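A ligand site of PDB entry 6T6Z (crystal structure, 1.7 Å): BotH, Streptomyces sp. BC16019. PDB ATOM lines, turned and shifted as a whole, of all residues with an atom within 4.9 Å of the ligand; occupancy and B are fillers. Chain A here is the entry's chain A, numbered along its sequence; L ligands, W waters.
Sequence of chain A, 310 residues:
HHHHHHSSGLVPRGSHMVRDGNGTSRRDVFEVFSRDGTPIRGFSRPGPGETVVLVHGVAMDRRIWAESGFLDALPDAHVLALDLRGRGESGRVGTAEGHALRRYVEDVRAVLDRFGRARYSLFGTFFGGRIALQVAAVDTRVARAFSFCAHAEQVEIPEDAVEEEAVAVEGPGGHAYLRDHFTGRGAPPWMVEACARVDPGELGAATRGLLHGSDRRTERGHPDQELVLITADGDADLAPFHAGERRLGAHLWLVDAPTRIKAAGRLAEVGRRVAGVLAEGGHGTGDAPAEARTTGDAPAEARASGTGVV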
ATOM      1  N   VAL A  58     -19.665 -17.345  -3.191  1.00  0.00           N
ATOM      2  CA  VAL A  58     -19.378 -18.270  -2.091  1.00  0.00           C
ATOM      3  C   VAL A  58     -17.910 -18.240  -1.717  1.00  0.00           C
ATOM      4  O   VAL A  58     -17.553 -18.162  -0.527  1.00  0.00           O
ATOM      5  CB  VAL A  58     -19.800 -19.698  -2.488  1.00  0.00           C
ATOM      6  CG1 VAL A  58     -19.336 -20.707  -1.435  1.00  0.00           C
ATOM      7  CG2 VAL A  58     -21.298 -19.780  -2.678  1.00  0.00           C
ATOM      8  N   ALA A  59     -17.034 -18.397  -2.701  1.00  0.00           N
ATOM      9  CA  ALA A  59     -15.593 -18.488  -2.459  1.00  0.00           C
ATOM     10  C   ALA A  59     -14.922 -17.138  -2.666  1.00  0.00           C
ATOM     11  O   ALA A  59     -13.827 -17.047  -3.238  1.00  0.00           O
ATOM     12  CB  ALA A  59     -14.967 -19.538  -3.364  1.00  0.00           C
ATOM     13  N   PHE A 126     -22.653 -14.421  -9.058  1.00  0.00           N
ATOM     14  CA  PHE A 126     -22.854 -15.873  -8.948  1.00  0.00           C
ATOM     15  C   PHE A 126     -23.862 -16.138  -7.845  1.00  0.00           C
ATOM     16  O   PHE A 126     -24.996 -15.634  -7.945  1.00  0.00           O
ATOM     17  CB  PHE A 126     -21.482 -16.528  -8.803  1.00  0.00           C
ATOM     18  CG  PHE A 126     -20.605 -16.343 -10.017  1.00  0.00           C
ATOM     19  CD1 PHE A 126     -20.830 -17.083 -11.169  1.00  0.00           C
ATOM     20  CD2 PHE A 126     -19.576 -15.418 -10.010  1.00  0.00           C
ATOM     21  CE1 PHE A 126     -20.042 -16.912 -12.289  1.00  0.00           C
ATOM     22  CE2 PHE A 126     -18.779 -15.244 -11.126  1.00  0.00           C
ATOM     23  CZ  PHE A 126     -19.014 -15.993 -12.274  1.00  0.00           C
ATOM     24  N   PHE A 127     -23.555 -16.910  -6.804  1.00  0.00           N
ATOM     25  CA  PHE A 127     -24.580 -17.120  -5.798  1.00  0.00           C
ATOM     26  C   PHE A 127     -24.963 -15.831  -5.080  1.00  0.00           C
ATOM     27  O   PHE A 127     -26.063 -15.735  -4.542  1.00  0.00           O
ATOM     28  CB  PHE A 127     -24.154 -18.152  -4.768  1.00  0.00           C
ATOM     29  CG  PHE A 127     -25.295 -18.630  -3.927  1.00  0.00           C
ATOM     30  CD1 PHE A 127     -26.306 -19.392  -4.489  1.00  0.00           C
ATOM     31  CD2 PHE A 127     -25.399 -18.278  -2.597  1.00  0.00           C
ATOM     32  CE1 PHE A 127     -27.380 -19.808  -3.734  1.00  0.00           C
ATOM     33  CE2 PHE A 127     -26.465 -18.696  -1.830  1.00  0.00           C
ATOM     34  CZ  PHE A 127     -27.458 -19.463  -2.407  1.00  0.00           C
ATOM     35  N   ARG A 130     -28.076 -14.784  -6.665  1.00  0.00           N
ATOM     36  CA  ARG A 130     -29.249 -15.430  -6.094  1.00  0.00           C
ATOM     37  C   ARG A 130     -29.652 -14.754  -4.798  1.00  0.00           C
ATOM     38  O   ARG A 130     -30.839 -14.535  -4.540  1.00  0.00           O
ATOM     39  CB  ARG A 130     -28.964 -16.914  -5.850  1.00  0.00           C
ATOM     40  CG  ARG A 130     -28.582 -17.724  -7.074  1.00  0.00           C
ATOM     41  CD  ARG A 130     -29.790 -18.123  -7.907  1.00  0.00           C
ATOM     42  NE  ARG A 130     -30.643 -19.118  -7.245  1.00  0.00           N
ATOM     43  CZ  ARG A 130     -31.604 -19.809  -7.861  1.00  0.00           C
ATOM     44  NH1 ARG A 130     -31.829 -19.603  -9.150  1.00  0.00           N
ATOM     45  NH2 ARG A 130     -32.330 -20.690  -7.201  1.00  0.00           N
ATOM     46  N   CYS A 149     -24.506 -13.610 -13.618  1.00  0.00           N
ATOM     47  CA  CYS A 149     -24.206 -15.009 -13.900  1.00  0.00           C
ATOM     48  C   CYS A 149     -24.944 -15.949 -12.946  1.00  0.00           C
ATOM     49  O   CYS A 149     -24.443 -17.017 -12.591  1.00  0.00           O
ATOM     50  CB  CYS A 149     -22.698 -15.278 -13.876  1.00  0.00           C
ATOM     51  SG  CYS A 149     -21.834 -14.513 -15.293  1.00  0.00           S
ATOM     52  N   ALA A 150     -26.149 -15.562 -12.549  1.00  0.00           N
ATOM     53  CA  ALA A 150     -27.066 -16.450 -11.862  1.00  0.00           C
ATOM     54  C   ALA A 150     -28.478 -16.051 -12.257  1.00  0.00           C
ATOM     55  O   ALA A 150     -28.763 -14.863 -12.438  1.00  0.00           O
ATOM     56  CB  ALA A 150     -26.898 -16.396 -10.342  1.00  0.00           C
ATOM     57  N   VAL A 155     -33.993 -24.792  -9.196  1.00  0.00           N
ATOM     58  CA  VAL A 155     -32.941 -25.686  -9.653  1.00  0.00           C
ATOM     59  C   VAL A 155     -33.031 -26.987  -8.875  1.00  0.00           C
ATOM     60  O   VAL A 155     -33.492 -27.022  -7.735  1.00  0.00           O
ATOM     61  CB  VAL A 155     -31.542 -25.055  -9.508  1.00  0.00           C
ATOM     62  CG1 VAL A 155     -31.415 -23.856 -10.423  1.00  0.00           C
ATOM     63  CG2 VAL A 155     -31.278 -24.647  -8.063  1.00  0.00           C
ATOM     64  N   GLU A 156     -32.599 -28.076  -9.513  1.00  0.00           N
ATOM     65  CA  GLU A 156     -32.437 -29.360  -8.837  1.00  0.00           C
ATOM     66  C   GLU A 156     -30.991 -29.470  -8.383  1.00  0.00           C
ATOM     67  O   GLU A 156     -30.064 -29.378  -9.197  1.00  0.00           O
ATOM     68  CB  GLU A 156     -32.807 -30.510  -9.761  1.00  0.00           C
ATOM     69  CG  GLU A 156     -34.290 -30.592 -10.076  1.00  0.00           C
ATOM     70  CD  GLU A 156     -34.631 -31.807 -10.920  1.00  0.00           C
ATOM     71  OE1 GLU A 156     -33.697 -32.463 -11.433  1.00  0.00           O
ATOM     72  OE2 GLU A 156     -35.837 -32.102 -11.081  1.00  0.00           O
ATOM     73  N   ILE A 157     -30.790 -29.634  -7.077  1.00  0.00           N
ATOM     74  CA  ILE A 157     -29.456 -29.693  -6.506  1.00  0.00           C
ATOM     75  C   ILE A 157     -29.163 -31.147  -6.137  1.00  0.00           C
ATOM     76  O   ILE A 157     -29.832 -31.697  -5.257  1.00  0.00           O
ATOM     77  CB  ILE A 157     -29.330 -28.778  -5.280  1.00  0.00           C
ATOM     78  CG1 ILE A 157     -29.556 -27.323  -5.705  1.00  0.00           C
ATOM     79  CG2 ILE A 157     -27.965 -28.945  -4.624  1.00  0.00           C
ATOM     80  CD1 ILE A 157     -29.460 -26.313  -4.586  1.00  0.00           C
ATOM     81  N   PRO A 158     -28.195 -31.808  -6.790  1.00  0.00           N
ATOM     82  CA  PRO A 158     -27.912 -33.211  -6.445  1.00  0.00           C
ATOM     83  C   PRO A 158     -27.202 -33.290  -5.090  1.00  0.00           C
ATOM     84  O   PRO A 158     -26.107 -32.754  -4.920  1.00  0.00           O
ATOM     85  CB  PRO A 158     -27.017 -33.686  -7.594  1.00  0.00           C
ATOM     86  CG  PRO A 158     -26.534 -32.461  -8.304  1.00  0.00           C
ATOM     87  CD  PRO A 158     -27.212 -31.248  -7.721  1.00  0.00           C
ATOM     88  N   ALA A 161     -23.527 -34.936  -5.194  1.00  0.00           N
ATOM     89  CA  ALA A 161     -22.466 -34.144  -5.803  1.00  0.00           C
ATOM     90  C   ALA A 161     -22.090 -32.952  -4.935  1.00  0.00           C
ATOM     91  O   ALA A 161     -20.906 -32.601  -4.834  1.00  0.00           O
ATOM     92  CB  ALA A 161     -22.889 -33.676  -7.200  1.00  0.00           C
ATOM     93  N   VAL A 162     -23.073 -32.303  -4.318  1.00  0.00           N
ATOM     94  CA  VAL A 162     -22.764 -31.151  -3.474  1.00  0.00           C
ATOM     95  C   VAL A 162     -21.979 -31.576  -2.250  1.00  0.00           C
ATOM     96  O   VAL A 162     -21.022 -30.913  -1.857  1.00  0.00           O
ATOM     97  CB  VAL A 162     -24.057 -30.402  -3.100  1.00  0.00           C
ATOM     98  CG1 VAL A 162     -23.786 -29.392  -1.990  1.00  0.00           C
ATOM     99  CG2 VAL A 162     -24.622 -29.708  -4.338  1.00  0.00           C
ATOM    100  N   GLU A 165     -18.523 -32.149  -3.284  1.00  0.00           N
ATOM    101  CA  GLU A 165     -17.802 -30.892  -3.469  1.00  0.00           C
ATOM    102  C   GLU A 165     -17.446 -30.267  -2.127  1.00  0.00           C
ATOM    103  O   GLU A 165     -16.361 -29.680  -1.982  1.00  0.00           O
ATOM    104  CB  GLU A 165     -18.645 -29.930  -4.302  1.00  0.00           C
ATOM    105  CG  GLU A 165     -17.954 -28.636  -4.651  1.00  0.00           C
ATOM    106  CD  GLU A 165     -18.187 -28.231  -6.091  1.00  0.00           C
ATOM    107  OE1 GLU A 165     -17.467 -28.739  -6.965  1.00  0.00           O
ATOM    108  OE2 GLU A 165     -19.108 -27.428  -6.334  1.00  0.00           O
ATOM    109  N   TYR A 177      -7.668 -27.197  -4.913  1.00  0.00           N
ATOM    110  CA  TYR A 177      -8.760 -27.720  -5.716  1.00  0.00           C
ATOM    111  C   TYR A 177      -9.513 -26.612  -6.430  1.00  0.00           C
ATOM    112  O   TYR A 177      -9.696 -26.660  -7.656  1.00  0.00           O
ATOM    113  CB  TYR A 177      -9.699 -28.519  -4.799  1.00  0.00           C
ATOM    114  CG  TYR A 177     -10.994 -28.997  -5.423  1.00  0.00           C
ATOM    115  CD1 TYR A 177     -11.058 -30.210  -6.101  1.00  0.00           C
ATOM    116  CD2 TYR A 177     -12.159 -28.264  -5.301  1.00  0.00           C
ATOM    117  CE1 TYR A 177     -12.250 -30.665  -6.660  1.00  0.00           C
ATOM    118  CE2 TYR A 177     -13.360 -28.698  -5.857  1.00  0.00           C
ATOM    119  CZ  TYR A 177     -13.392 -29.902  -6.538  1.00  0.00           C
ATOM    120  OH  TYR A 177     -14.576 -30.335  -7.080  1.00  0.00           O
ATOM    121  N   LEU A 178      -9.946 -25.599  -5.685  1.00  0.00           N
ATOM    122  CA  LEU A 178     -10.668 -24.480  -6.287  1.00  0.00           C
ATOM    123  C   LEU A 178      -9.772 -23.674  -7.215  1.00  0.00           C
ATOM    124  O   LEU A 178     -10.195 -23.275  -8.313  1.00  0.00           O
ATOM    125  CB  LEU A 178     -11.235 -23.566  -5.190  1.00  0.00           C
ATOM    126  CG  LEU A 178     -12.420 -24.125  -4.416  1.00  0.00           C
ATOM    127  CD1 LEU A 178     -12.816 -23.195  -3.277  1.00  0.00           C
ATOM    128  CD2 LEU A 178     -13.606 -24.348  -5.339  1.00  0.00           C
ATOM    129  N   HIS A 181      -9.389 -25.576 -10.445  1.00  0.00           N
ATOM    130  CA  HIS A 181     -10.636 -25.584 -11.197  1.00  0.00           C
ATOM    131  C   HIS A 181     -10.881 -24.246 -11.890  1.00  0.00           C
ATOM    132  O   HIS A 181     -11.238 -24.193 -13.068  1.00  0.00           O
ATOM    133  CB  HIS A 181     -11.809 -25.917 -10.275  1.00  0.00           C
ATOM    134  CG  HIS A 181     -13.124 -26.033 -10.978  1.00  0.00           C
ATOM    135  ND1 HIS A 181     -14.071 -25.027 -10.956  1.00  0.00           N
ATOM    136  CD2 HIS A 181     -13.662 -27.041 -11.708  1.00  0.00           C
ATOM    137  CE1 HIS A 181     -15.134 -25.411 -11.650  1.00  0.00           C
ATOM    138  NE2 HIS A 181     -14.902 -26.630 -12.116  1.00  0.00           N
ATOM    139  N   PHE A 182     -10.679 -23.145 -11.158  1.00  0.00           N
ATOM    140  CA  PHE A 182     -10.981 -21.832 -11.712  1.00  0.00           C
ATOM    141  C   PHE A 182      -9.931 -21.402 -12.711  1.00  0.00           C
ATOM    142  O   PHE A 182     -10.260 -20.775 -13.726  1.00  0.00           O
ATOM    143  CB  PHE A 182     -11.110 -20.814 -10.582  1.00  0.00           C
ATOM    144  CG  PHE A 182     -12.383 -20.934  -9.822  1.00  0.00           C
ATOM    145  CD1 PHE A 182     -13.563 -21.131 -10.498  1.00  0.00           C
ATOM    146  CD2 PHE A 182     -12.410 -20.887  -8.440  1.00  0.00           C
ATOM    147  CE1 PHE A 182     -14.733 -21.264  -9.839  1.00  0.00           C
ATOM    148  CE2 PHE A 182     -13.606 -21.015  -7.754  1.00  0.00           C
ATOM    149  CZ  PHE A 182     -14.765 -21.210  -8.452  1.00  0.00           C
ATOM    150  N   MET A 191     -10.490 -13.747  -9.009  1.00  0.00           N
ATOM    151  CA  MET A 191     -11.427 -14.794  -8.634  1.00  0.00           C
ATOM    152  C   MET A 191     -10.690 -16.038  -8.177  1.00  0.00           C
ATOM    153  O   MET A 191     -11.080 -16.686  -7.207  1.00  0.00           O
ATOM    154  CB  MET A 191     -12.358 -15.085  -9.813  1.00  0.00           C
ATOM    155  CG  MET A 191     -13.436 -16.106  -9.570  1.00  0.00           C
ATOM    156  SD  MET A 191     -14.647 -16.063 -10.898  1.00  0.00           S
ATOM    157  CE  MET A 191     -15.542 -17.564 -10.550  1.00  0.00           C
ATOM    158  N   THR A 207     -20.959 -24.703   1.142  1.00  0.00           N
ATOM    159  CA  THR A 207     -21.371 -25.634   0.104  1.00  0.00           C
ATOM    160  C   THR A 207     -22.552 -26.485   0.581  1.00  0.00           C
ATOM    161  O   THR A 207     -23.558 -26.626  -0.126  1.00  0.00           O
ATOM    162  CB  THR A 207     -20.183 -26.508  -0.313  1.00  0.00           C
ATOM    163  OG1 THR A 207     -19.157 -25.678  -0.870  1.00  0.00           O
ATOM    164  CG2 THR A 207     -20.606 -27.539  -1.339  1.00  0.00           C
ATOM    165  N   LEU A 210     -26.074 -24.858   0.722  1.00  0.00           N
ATOM    166  CA  LEU A 210     -26.891 -24.778  -0.479  1.00  0.00           C
ATOM    167  C   LEU A 210     -28.031 -25.793  -0.463  1.00  0.00           C
ATOM    168  O   LEU A 210     -28.999 -25.627  -1.196  1.00  0.00           O
ATOM    169  CB  LEU A 210     -26.026 -25.003  -1.716  1.00  0.00           C
ATOM    170  CG  LEU A 210     -24.906 -23.976  -1.926  1.00  0.00           C
ATOM    171  CD1 LEU A 210     -23.979 -24.424  -3.063  1.00  0.00           C
ATOM    172  CD2 LEU A 210     -25.475 -22.591  -2.223  1.00  0.00           C
ATOM    173  N   SER A 214     -31.637 -23.032  -1.129  1.00  0.00           N
ATOM    174  CA  SER A 214     -31.148 -22.315  -2.302  1.00  0.00           C
ATOM    175  C   SER A 214     -31.739 -22.846  -3.607  1.00  0.00           C
ATOM    176  O   SER A 214     -31.476 -22.249  -4.666  1.00  0.00           O
ATOM    177  CB  SER A 214     -29.628 -22.386  -2.391  1.00  0.00           C
ATOM    178  OG  SER A 214     -29.210 -23.598  -2.986  1.00  0.00           O
ATOM    179  N   ARG A 260     -19.959 -18.859 -18.076  1.00  0.00           N
ATOM    180  CA  ARG A 260     -20.255 -17.962 -16.954  1.00  0.00           C
ATOM    181  C   ARG A 260     -18.989 -17.558 -16.212  1.00  0.00           C
ATOM    182  O   ARG A 260     -18.840 -16.401 -15.809  1.00  0.00           O
ATOM    183  CB  ARG A 260     -21.224 -18.623 -15.985  1.00  0.00           C
ATOM    184  CG  ARG A 260     -22.626 -18.750 -16.515  1.00  0.00           C
ATOM    185  CD  ARG A 260     -23.556 -19.435 -15.535  1.00  0.00           C
ATOM    186  NE  ARG A 260     -24.756 -19.895 -16.212  1.00  0.00           N
ATOM    187  CZ  ARG A 260     -25.654 -20.724 -15.692  1.00  0.00           C
ATOM    188  NH1 ARG A 260     -25.503 -21.201 -14.466  1.00  0.00           N
ATOM    189  NH2 ARG A 260     -26.714 -21.083 -16.418  1.00  0.00           N
ATOM    190  N   ILE A 261     -18.075 -18.508 -16.006  1.00  0.00           N
ATOM    191  CA  ILE A 261     -16.838 -18.190 -15.308  1.00  0.00           C
ATOM    192  C   ILE A 261     -16.023 -17.174 -16.097  1.00  0.00           C
ATOM    193  O   ILE A 261     -15.476 -16.217 -15.543  1.00  0.00           O
ATOM    194  CB  ILE A 261     -16.024 -19.462 -15.017  1.00  0.00           C
ATOM    195  CG1 ILE A 261     -16.661 -20.228 -13.857  1.00  0.00           C
ATOM    196  CG2 ILE A 261     -14.568 -19.115 -14.729  1.00  0.00           C
ATOM    197  CD1 ILE A 261     -16.018 -21.561 -13.564  1.00  0.00           C
HETATM  198  C1  LIG L   1     -24.588 -21.434  -8.406  1.00  0.00           C
HETATM  199  C2  LIG L   1     -27.117 -21.360  -8.258  1.00  0.00           C
HETATM  200  C3  LIG L   1     -27.175 -22.668  -5.844  1.00  0.00           C
HETATM  201  C4  LIG L   1     -25.965 -22.402  -6.474  1.00  0.00           C
HETATM  202  C5  LIG L   1     -24.323 -19.965  -8.636  1.00  0.00           C
HETATM  203  C6  LIG L   1     -20.480 -23.018 -12.330  1.00  0.00           C
HETATM  204  C7  LIG L   1     -20.295 -25.917  -9.341  1.00  0.00           C
HETATM  205  C8  LIG L   1     -21.980 -27.865  -9.154  1.00  0.00           C
HETATM  206  C9  LIG L   1     -21.920 -29.373  -9.012  1.00  0.00           C
HETATM  207  C10 LIG L   1     -21.124 -29.820  -7.765  1.00  0.00           C
HETATM  208  C11 LIG L   1     -21.211 -29.956 -10.247  1.00  0.00           C
HETATM  209  C12 LIG L   1     -23.329 -29.949  -8.927  1.00  0.00           C
HETATM  210  C13 LIG L   1     -22.892 -27.017  -8.076  1.00  0.00           C
HETATM  211  C14 LIG L   1     -24.759 -26.339  -9.688  1.00  0.00           C
HETATM  212  C15 LIG L   1     -24.768 -24.860 -10.277  1.00  0.00           C
HETATM  213  C16 LIG L   1     -24.508 -22.307  -9.732  1.00  0.00           C
HETATM  214  C17 LIG L   1     -25.890 -21.725  -7.690  1.00  0.00           C
HETATM  215  C18 LIG L   1     -28.327 -21.619  -7.636  1.00  0.00           C
HETATM  216  C19 LIG L   1     -28.375 -22.281  -6.417  1.00  0.00           C
HETATM  217  C20 LIG L   1     -23.301 -21.816 -10.607  1.00  0.00           C
HETATM  218  C21 LIG L   1     -20.916 -21.841 -11.424  1.00  0.00           C
HETATM  219  C22 LIG L   1     -21.441 -23.218 -13.468  1.00  0.00           C
HETATM  220  C23 LIG L   1     -21.389 -23.097 -15.804  1.00  0.00           C
HETATM  221  C24 LIG L   1     -19.805 -21.245 -10.627  1.00  0.00           C
HETATM  222  C25 LIG L   1     -17.824 -20.842  -9.693  1.00  0.00           C
HETATM  223  C26 LIG L   1     -18.501 -19.803  -9.141  1.00  0.00           C
HETATM  224  C27 LIG L   1     -26.294 -26.623  -9.405  1.00  0.00           C
HETATM  225  C28 LIG L   1     -26.431 -27.976  -8.659  1.00  0.00           C
HETATM  226  C29 LIG L   1     -26.919 -25.537  -8.510  1.00  0.00           C
HETATM  227  C30 LIG L   1     -27.134 -26.702 -10.679  1.00  0.00           C
HETATM  228  C31 LIG L   1     -18.971 -25.214  -8.871  1.00  0.00           C
HETATM  229  C32 LIG L   1     -17.596 -25.930  -8.934  1.00  0.00           C
HETATM  230  C33 LIG L   1     -16.408 -25.069  -8.483  1.00  0.00           C
HETATM  231  C34 LIG L   1     -14.891 -27.768  -8.683  1.00  0.00           C
HETATM  232  C35 LIG L   1     -19.580 -23.455  -7.070  1.00  0.00           C
HETATM  233  C36 LIG L   1     -20.014 -23.201  -5.619  1.00  0.00           C
HETATM  234  C37 LIG L   1     -18.823 -23.174  -4.629  1.00  0.00           C
HETATM  235  C38 LIG L   1     -17.469 -22.706  -5.130  1.00  0.00           C
HETATM  236  C39 LIG L   1     -18.683 -24.647  -4.201  1.00  0.00           C
HETATM  237  C40 LIG L   1     -20.086 -25.254  -4.365  1.00  0.00           C
HETATM  238  C41 LIG L   1     -22.077 -24.795  -5.904  1.00  0.00           C
HETATM  239  C42 LIG L   1     -22.817 -26.181  -5.630  1.00  0.00           C
HETATM  240  N1  LIG L   1     -20.695 -27.170  -8.870  1.00  0.00           N
HETATM  241  N2  LIG L   1     -23.983 -26.409  -8.421  1.00  0.00           N
HETATM  242  N3  LIG L   1     -24.498 -23.759  -9.400  1.00  0.00           N
HETATM  243  N4  LIG L   1     -22.026 -22.345 -10.575  1.00  0.00           N
HETATM  244  N5  LIG L   1     -18.568 -21.687 -10.558  1.00  0.00           N
HETATM  245  N6  LIG L   1     -19.357 -24.774  -7.499  1.00  0.00           N
HETATM  246  N7  LIG L   1     -20.836 -24.402  -5.350  1.00  0.00           N
HETATM  247  N8  LIG L   1     -22.312 -26.962  -6.758  1.00  0.00           N
HETATM  248  O1  LIG L   1     -21.014 -25.285 -10.099  1.00  0.00           O
HETATM  249  O2  LIG L   1     -21.138 -22.492 -14.613  1.00  0.00           O
HETATM  250  O3  LIG L   1     -22.431 -23.926 -13.469  1.00  0.00           O
HETATM  251  O4  LIG L   1     -23.443 -20.894 -11.405  1.00  0.00           O
HETATM  252  O5  LIG L   1     -25.017 -24.634 -11.439  1.00  0.00           O
HETATM  253  O6  LIG L   1     -22.550 -24.037  -6.745  1.00  0.00           O
HETATM  254  O7  LIG L   1     -19.441 -22.515  -7.841  1.00  0.00           O
HETATM  255  S1  LIG L   1     -20.105 -19.809  -9.661  1.00  0.00           S
HETATM  256  S2  LIG L   1     -14.966 -26.106  -7.903  1.00  0.00           S
HETATM  257  O   HOH W   1     -26.963 -22.624 -12.421  1.00  0.00           O
HETATM  258  O   HOH W   2     -18.968 -21.481 -16.301  1.00  0.00           O
HETATM  259  O   HOH W   3     -23.803 -22.454 -18.112  1.00  0.00           O
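Merely in contact with the ligand: Phe 126 (3.2 Å), Phe 127 (3.6 Å), Arg 130 (3.4 Å), Glu 156 (3.9 Å), Pro 158 (3.5 Å), Tyr 177 (3.0 Å), Leu 178 (3.4 Å), Phe 182 (3.1 Å), Met 191 (3.97 Å), Thr 207 (3.5 Å), Leu 210 (3.3 Å), Ser 214 (3.6 Å), Arg 260 (3.7 Å) and Ile 261 (3.9 Å). Hydrophobic or aromatic side chains within 4 Å of the ligand: Phe 126, Phe 127, Pro 158, Tyr 177, Leu 178, His 181, Phe 182, Met 191, Leu 210 and Ile 261. Of the 24 residues printed, 16 come within 4 Å of the ligand.
N6 of the ligand lies within hydrogen-bond range of OE2 of Glu 165 (2.9 Å). ND1 of His 181 sits close to S2 of the ligand (3.4 Å).
Water W2 lies within hydrogen-bond range of O2 of the ligand, N of Ile 261 and N of Arg 260. Water W1 lies within hydrogen-bond range of NH1 of Arg 260 (2.9 Å) and O5 of the ligand (3.0 Å).
The side-chain carboxylate (OE1) of Glu 165 is in hydrogen-bond range of the side-chain hydroxyl (OH) of Tyr 177 (3.3 Å). The side-chain hydroxyl of Ser 214 is in hydrogen-bond range of the backbone carbonyl oxygen of Leu 210, 2.7 Å away. NH2 of Arg 130 lies within hydrogen-bond range of O of Ser 214, 3.1 Å away. The backbone carbonyl oxygen (O) of Arg 260 is in hydrogen-bond range of the side-chain sulfur (SG) of Cys 149.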
